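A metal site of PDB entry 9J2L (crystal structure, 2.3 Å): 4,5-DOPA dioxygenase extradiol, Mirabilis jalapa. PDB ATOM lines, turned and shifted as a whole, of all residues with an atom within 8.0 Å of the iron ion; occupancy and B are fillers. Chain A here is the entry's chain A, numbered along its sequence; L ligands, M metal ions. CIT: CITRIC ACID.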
ATOM      1  N   ASN A   8     -21.255  13.419 -12.314  1.00  0.00           N
ATOM      2  CA  ASN A   8     -21.725  12.956 -13.605  1.00  0.00           C
ATOM      3  C   ASN A   8     -20.645  13.291 -14.634  1.00  0.00           C
ATOM      4  O   ASN A   8     -20.117  14.405 -14.638  1.00  0.00           O
ATOM      5  CB  ASN A   8     -23.040  13.634 -13.985  1.00  0.00           C
ATOM      6  CG  ASN A   8     -24.210  13.206 -13.092  1.00  0.00           C
ATOM      7  OD1 ASN A   8     -25.229  12.749 -13.570  1.00  0.00           O
ATOM      8  ND2 ASN A   8     -24.063  13.409 -11.800  1.00  0.00           N
ATOM      9  N   HIS A   9     -20.309  12.326 -15.488  1.00  0.00           N
ATOM     10  CA  HIS A   9     -19.335  12.649 -16.509  1.00  0.00           C
ATOM     11  C   HIS A   9     -19.973  13.443 -17.631  1.00  0.00           C
ATOM     12  O   HIS A   9     -19.257  14.155 -18.341  1.00  0.00           O
ATOM     13  CB  HIS A   9     -18.675  11.374 -17.079  1.00  0.00           C
ATOM     14  CG  HIS A   9     -19.612  10.217 -17.267  1.00  0.00           C
ATOM     15  ND1 HIS A   9     -19.866   9.290 -16.272  1.00  0.00           N
ATOM     16  CD2 HIS A   9     -20.359   9.839 -18.339  1.00  0.00           C
ATOM     17  CE1 HIS A   9     -20.732   8.397 -16.722  1.00  0.00           C
ATOM     18  NE2 HIS A   9     -21.046   8.699 -17.968  1.00  0.00           N
ATOM     19  N   GLY A  10     -21.290  13.337 -17.784  1.00  0.00           N
ATOM     20  CA  GLY A  10     -22.037  14.140 -18.726  1.00  0.00           C
ATOM     21  C   GLY A  10     -21.817  13.795 -20.201  1.00  0.00           C
ATOM     22  O   GLY A  10     -21.222  12.791 -20.572  1.00  0.00           O
ATOM     23  N   ASP A  11     -22.339  14.681 -21.027  1.00  0.00           N
ATOM     24  CA  ASP A  11     -22.381  14.513 -22.462  1.00  0.00           C
ATOM     25  C   ASP A  11     -21.045  14.895 -23.078  1.00  0.00           C
ATOM     26  O   ASP A  11     -20.648  16.060 -22.971  1.00  0.00           O
ATOM     27  CB  ASP A  11     -23.527  15.395 -23.017  1.00  0.00           C
ATOM     28  CG  ASP A  11     -23.714  15.284 -24.530  1.00  0.00           C
ATOM     29  OD1 ASP A  11     -22.972  14.578 -25.231  1.00  0.00           O
ATOM     30  OD2 ASP A  11     -24.646  15.953 -25.039  1.00  0.00           O
ATOM     31  N   PRO A  12     -20.335  13.976 -23.728  1.00  0.00           N
ATOM     32  CA  PRO A  12     -19.044  14.323 -24.352  1.00  0.00           C
ATOM     33  C   PRO A  12     -19.115  15.528 -25.288  1.00  0.00           C
ATOM     34  O   PRO A  12     -18.116  16.222 -25.492  1.00  0.00           O
ATOM     35  CB  PRO A  12     -18.659  13.049 -25.097  1.00  0.00           C
ATOM     36  CG  PRO A  12     -19.340  11.958 -24.328  1.00  0.00           C
ATOM     37  CD  PRO A  12     -20.659  12.547 -23.880  1.00  0.00           C
ATOM     38  N   SER A  45     -16.495   3.734 -12.175  1.00  0.00           N
ATOM     39  CA  SER A  45     -16.917   4.080 -13.532  1.00  0.00           C
ATOM     40  C   SER A  45     -18.218   3.378 -13.889  1.00  0.00           C
ATOM     41  O   SER A  45     -18.291   2.139 -13.866  1.00  0.00           O
ATOM     42  CB  SER A  45     -15.850   3.689 -14.546  1.00  0.00           C
ATOM     43  OG  SER A  45     -16.373   3.752 -15.860  1.00  0.00           O
ATOM     44  N   ALA A  46     -19.217   4.169 -14.290  1.00  0.00           N
ATOM     45  CA  ALA A  46     -20.437   3.565 -14.812  1.00  0.00           C
ATOM     46  C   ALA A  46     -20.193   2.812 -16.104  1.00  0.00           C
ATOM     47  O   ALA A  46     -21.028   2.003 -16.503  1.00  0.00           O
ATOM     48  CB  ALA A  46     -21.487   4.644 -15.053  1.00  0.00           C
ATOM     49  N   HIS A  47     -19.072   3.054 -16.788  1.00  0.00           N
ATOM     50  CA  HIS A  47     -18.865   2.487 -18.124  1.00  0.00           C
ATOM     51  C   HIS A  47     -17.893   1.322 -18.100  1.00  0.00           C
ATOM     52  O   HIS A  47     -17.437   0.892 -19.165  1.00  0.00           O
ATOM     53  CB  HIS A  47     -18.377   3.569 -19.100  1.00  0.00           C
ATOM     54  CG  HIS A  47     -19.465   4.492 -19.563  1.00  0.00           C
ATOM     55  ND1 HIS A  47     -20.043   4.404 -20.806  1.00  0.00           N
ATOM     56  CD2 HIS A  47     -20.076   5.533 -18.942  1.00  0.00           C
ATOM     57  CE1 HIS A  47     -20.972   5.327 -20.935  1.00  0.00           C
ATOM     58  NE2 HIS A  47     -21.016   6.025 -19.819  1.00  0.00           N
ATOM     59  N   ASP A  66     -14.594   5.359 -25.565  1.00  0.00           N
ATOM     60  CA  ASP A  66     -15.685   4.380 -25.657  1.00  0.00           C
ATOM     61  C   ASP A  66     -17.017   5.117 -25.748  1.00  0.00           C
ATOM     62  O   ASP A  66     -17.844   5.092 -24.842  1.00  0.00           O
ATOM     63  CB  ASP A  66     -15.657   3.417 -24.483  1.00  0.00           C
ATOM     64  CG  ASP A  66     -15.757   4.124 -23.134  1.00  0.00           C
ATOM     65  OD1 ASP A  66     -15.209   5.251 -22.980  1.00  0.00           O
ATOM     66  OD2 ASP A  66     -16.385   3.538 -22.229  1.00  0.00           O
ATOM     67  N   TYR A  70     -19.713  10.488 -32.166  1.00  0.00           N
ATOM     68  CA  TYR A  70     -19.448  11.853 -31.796  1.00  0.00           C
ATOM     69  C   TYR A  70     -18.557  12.509 -32.843  1.00  0.00           C
ATOM     70  O   TYR A  70     -18.010  11.817 -33.713  1.00  0.00           O
ATOM     71  CB  TYR A  70     -18.768  11.889 -30.424  1.00  0.00           C
ATOM     72  CG  TYR A  70     -19.735  11.563 -29.308  1.00  0.00           C
ATOM     73  CD1 TYR A  70     -20.073  10.244 -29.019  1.00  0.00           C
ATOM     74  CD2 TYR A  70     -20.340  12.569 -28.590  1.00  0.00           C
ATOM     75  CE1 TYR A  70     -20.966   9.943 -28.023  1.00  0.00           C
ATOM     76  CE2 TYR A  70     -21.256  12.288 -27.600  1.00  0.00           C
ATOM     77  CZ  TYR A  70     -21.567  10.980 -27.317  1.00  0.00           C
ATOM     78  OH  TYR A  70     -22.452  10.698 -26.320  1.00  0.00           O
ATOM     79  N   HIS A 112     -14.223   6.935 -20.707  1.00  0.00           N
ATOM     80  CA  HIS A 112     -14.542   8.359 -20.637  1.00  0.00           C
ATOM     81  C   HIS A 112     -15.292   8.741 -19.366  1.00  0.00           C
ATOM     82  O   HIS A 112     -15.310   9.928 -19.025  1.00  0.00           O
ATOM     83  CB  HIS A 112     -15.311   8.796 -21.883  1.00  0.00           C
ATOM     84  CG  HIS A 112     -16.759   8.419 -21.899  1.00  0.00           C
ATOM     85  ND1 HIS A 112     -17.207   7.245 -22.469  1.00  0.00           N
ATOM     86  CD2 HIS A 112     -17.863   9.085 -21.481  1.00  0.00           C
ATOM     87  CE1 HIS A 112     -18.524   7.191 -22.369  1.00  0.00           C
ATOM     88  NE2 HIS A 112     -18.944   8.297 -21.792  1.00  0.00           N
ATOM     89  N   ALA A 113     -15.867   7.781 -18.636  1.00  0.00           N
ATOM     90  CA  ALA A 113     -16.430   8.101 -17.328  1.00  0.00           C
ATOM     91  C   ALA A 113     -15.378   8.682 -16.400  1.00  0.00           C
ATOM     92  O   ALA A 113     -15.705   9.449 -15.497  1.00  0.00           O
ATOM     93  CB  ALA A 113     -17.039   6.853 -16.694  1.00  0.00           C
ATOM     94  N   SER A 163     -18.540   8.028 -10.835  1.00  0.00           N
ATOM     95  CA  SER A 163     -18.836   8.785 -12.052  1.00  0.00           C
ATOM     96  C   SER A 163     -19.953   8.078 -12.790  1.00  0.00           C
ATOM     97  O   SER A 163     -19.721   7.046 -13.425  1.00  0.00           O
ATOM     98  CB  SER A 163     -17.598   8.940 -12.939  1.00  0.00           C
ATOM     99  OG  SER A 163     -17.947   9.610 -14.131  1.00  0.00           O
ATOM    100  N   GLY A 164     -21.152   8.644 -12.714  1.00  0.00           N
ATOM    101  CA  GLY A 164     -22.321   8.054 -13.328  1.00  0.00           C
ATOM    102  C   GLY A 164     -23.200   9.089 -14.000  1.00  0.00           C
ATOM    103  O   GLY A 164     -22.703  10.058 -14.584  1.00  0.00           O
ATOM    104  N   GLY A 165     -24.509   8.903 -13.877  1.00  0.00           N
ATOM    105  CA  GLY A 165     -25.516   9.806 -14.381  1.00  0.00           C
ATOM    106  C   GLY A 165     -26.737   9.688 -13.504  1.00  0.00           C
ATOM    107  O   GLY A 165     -27.332   8.610 -13.395  1.00  0.00           O
ATOM    108  N   HIS A 168     -30.662   8.652 -15.860  1.00  0.00           N
ATOM    109  CA  HIS A 168     -29.978   8.112 -17.030  1.00  0.00           C
ATOM    110  C   HIS A 168     -30.900   7.135 -17.733  1.00  0.00           C
ATOM    111  O   HIS A 168     -30.691   5.925 -17.690  1.00  0.00           O
ATOM    112  CB  HIS A 168     -28.672   7.436 -16.611  1.00  0.00           C
ATOM    113  CG  HIS A 168     -27.799   7.026 -17.760  1.00  0.00           C
ATOM    114  ND1 HIS A 168     -26.922   7.900 -18.375  1.00  0.00           N
ATOM    115  CD2 HIS A 168     -27.640   5.829 -18.367  1.00  0.00           C
ATOM    116  CE1 HIS A 168     -26.270   7.253 -19.328  1.00  0.00           C
ATOM    117  NE2 HIS A 168     -26.691   6.000 -19.350  1.00  0.00           N
ATOM    118  N   GLU A 221     -26.379   0.895 -14.043  1.00  0.00           N
ATOM    119  CA  GLU A 221     -24.925   1.033 -13.986  1.00  0.00           C
ATOM    120  C   GLU A 221     -24.495   2.486 -13.823  1.00  0.00           C
ATOM    121  O   GLU A 221     -23.407   2.733 -13.291  1.00  0.00           O
ATOM    122  CB  GLU A 221     -24.272   0.398 -15.227  1.00  0.00           C
ATOM    123  CG  GLU A 221     -24.289   1.251 -16.482  1.00  0.00           C
ATOM    124  CD  GLU A 221     -25.704   1.518 -16.975  1.00  0.00           C
ATOM    125  OE1 GLU A 221     -26.563   0.629 -16.838  1.00  0.00           O
ATOM    126  OE2 GLU A 221     -25.965   2.643 -17.464  1.00  0.00           O
ATOM    127  N   HIS A 222     -25.327   3.448 -14.231  1.00  0.00           N
ATOM    128  CA  HIS A 222     -25.006   4.846 -14.027  1.00  0.00           C
ATOM    129  C   HIS A 222     -25.414   5.352 -12.648  1.00  0.00           C
ATOM    130  O   HIS A 222     -25.039   6.470 -12.265  1.00  0.00           O
ATOM    131  CB  HIS A 222     -25.646   5.726 -15.136  1.00  0.00           C
ATOM    132  CG  HIS A 222     -24.755   5.922 -16.330  1.00  0.00           C
ATOM    133  ND1 HIS A 222     -24.467   4.901 -17.211  1.00  0.00           N
ATOM    134  CD2 HIS A 222     -24.041   6.987 -16.751  1.00  0.00           C
ATOM    135  CE1 HIS A 222     -23.627   5.340 -18.138  1.00  0.00           C
ATOM    136  NE2 HIS A 222     -23.359   6.608 -17.883  1.00  0.00           N
ATOM    137  N   PHE A 252     -32.234  13.647 -18.871  1.00  0.00           N
ATOM    138  CA  PHE A 252     -30.965  13.296 -18.240  1.00  0.00           C
ATOM    139  C   PHE A 252     -30.608  14.363 -17.219  1.00  0.00           C
ATOM    140  O   PHE A 252     -30.595  15.563 -17.540  1.00  0.00           O
ATOM    141  CB  PHE A 252     -29.857  13.137 -19.274  1.00  0.00           C
ATOM    142  CG  PHE A 252     -29.996  11.918 -20.131  1.00  0.00           C
ATOM    143  CD1 PHE A 252     -30.892  11.878 -21.181  1.00  0.00           C
ATOM    144  CD2 PHE A 252     -29.227  10.788 -19.866  1.00  0.00           C
ATOM    145  CE1 PHE A 252     -31.014  10.739 -21.979  1.00  0.00           C
ATOM    146  CE2 PHE A 252     -29.342   9.646 -20.652  1.00  0.00           C
ATOM    147  CZ  PHE A 252     -30.253   9.623 -21.707  1.00  0.00           C
HETATM  148  C1  CIT L   1     -21.899   8.072 -24.059  1.00  0.00           C
HETATM  149  O1  CIT L   1     -21.736   6.942 -23.540  1.00  0.00           O
HETATM  150  O2  CIT L   1     -21.936   8.202 -25.312  1.00  0.00           O
HETATM  151  C2  CIT L   1     -22.059   9.289 -23.156  1.00  0.00           C
HETATM  152  C3  CIT L   1     -22.533   8.994 -21.717  1.00  0.00           C
HETATM  153  O7  CIT L   1     -21.495   8.678 -20.821  1.00  0.00           O
HETATM  154  C4  CIT L   1     -23.277  10.238 -21.255  1.00  0.00           C
HETATM  155  C5  CIT L   1     -23.688  10.122 -19.785  1.00  0.00           C
HETATM  156  O3  CIT L   1     -24.246  11.110 -19.282  1.00  0.00           O
HETATM  157  O4  CIT L   1     -23.476   9.100 -19.079  1.00  0.00           O
HETATM  158  C6  CIT L   1     -23.525   7.857 -21.661  1.00  0.00           C
HETATM  159  O5  CIT L   1     -23.398   7.028 -20.712  1.00  0.00           O
HETATM  160  O6  CIT L   1     -24.433   7.766 -22.525  1.00  0.00           O
HETATM  161 FE    FE M   1     -22.229   7.592 -19.273  1.00  0.00          FE
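O5 of the ligand is bound to the iron ion (1.9 Å). The iron ion is bound by O4 of the ligand (2.0 Å). The iron ion is bound by O7 of the ligand (2.0 Å). The iron ion is bound by a ring nitrogen (NE2) of His 222, 2.0 Å away. The iron ion is bound by a ring nitrogen (NE2) of His 47 (2.1 Å). The iron ion is bound by a ring nitrogen (NE2) of His 9 (2.1 Å). The iron ion has six donor atoms within binding distance.
Three residues have an atom within 4 Å of the iron ion: His 9, His 47 and His 222.
ND1 of His 9 lies close to O of Gly 164, at 3.4 Å. The side-chain hydroxyl (OG) of Ser 45 sits at hydrogen-bond distance from the backbone NH (N) of His 47, at 2.9 Å. A ring nitrogen (ND1) of His 222 lies within hydrogen-bond range of the side-chain carboxylate of Glu 221 (2.7 Å). A ring nitrogen (ND1) of His 222 is in hydrogen-bond range of a ring nitrogen (NE2) of His 168 (3.3 Å). ND1 of His 9 lies within hydrogen-bond range of OG of Ser 163 (2.9 Å). N of Gly 165 lies within hydrogen-bond range of O of His 222.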
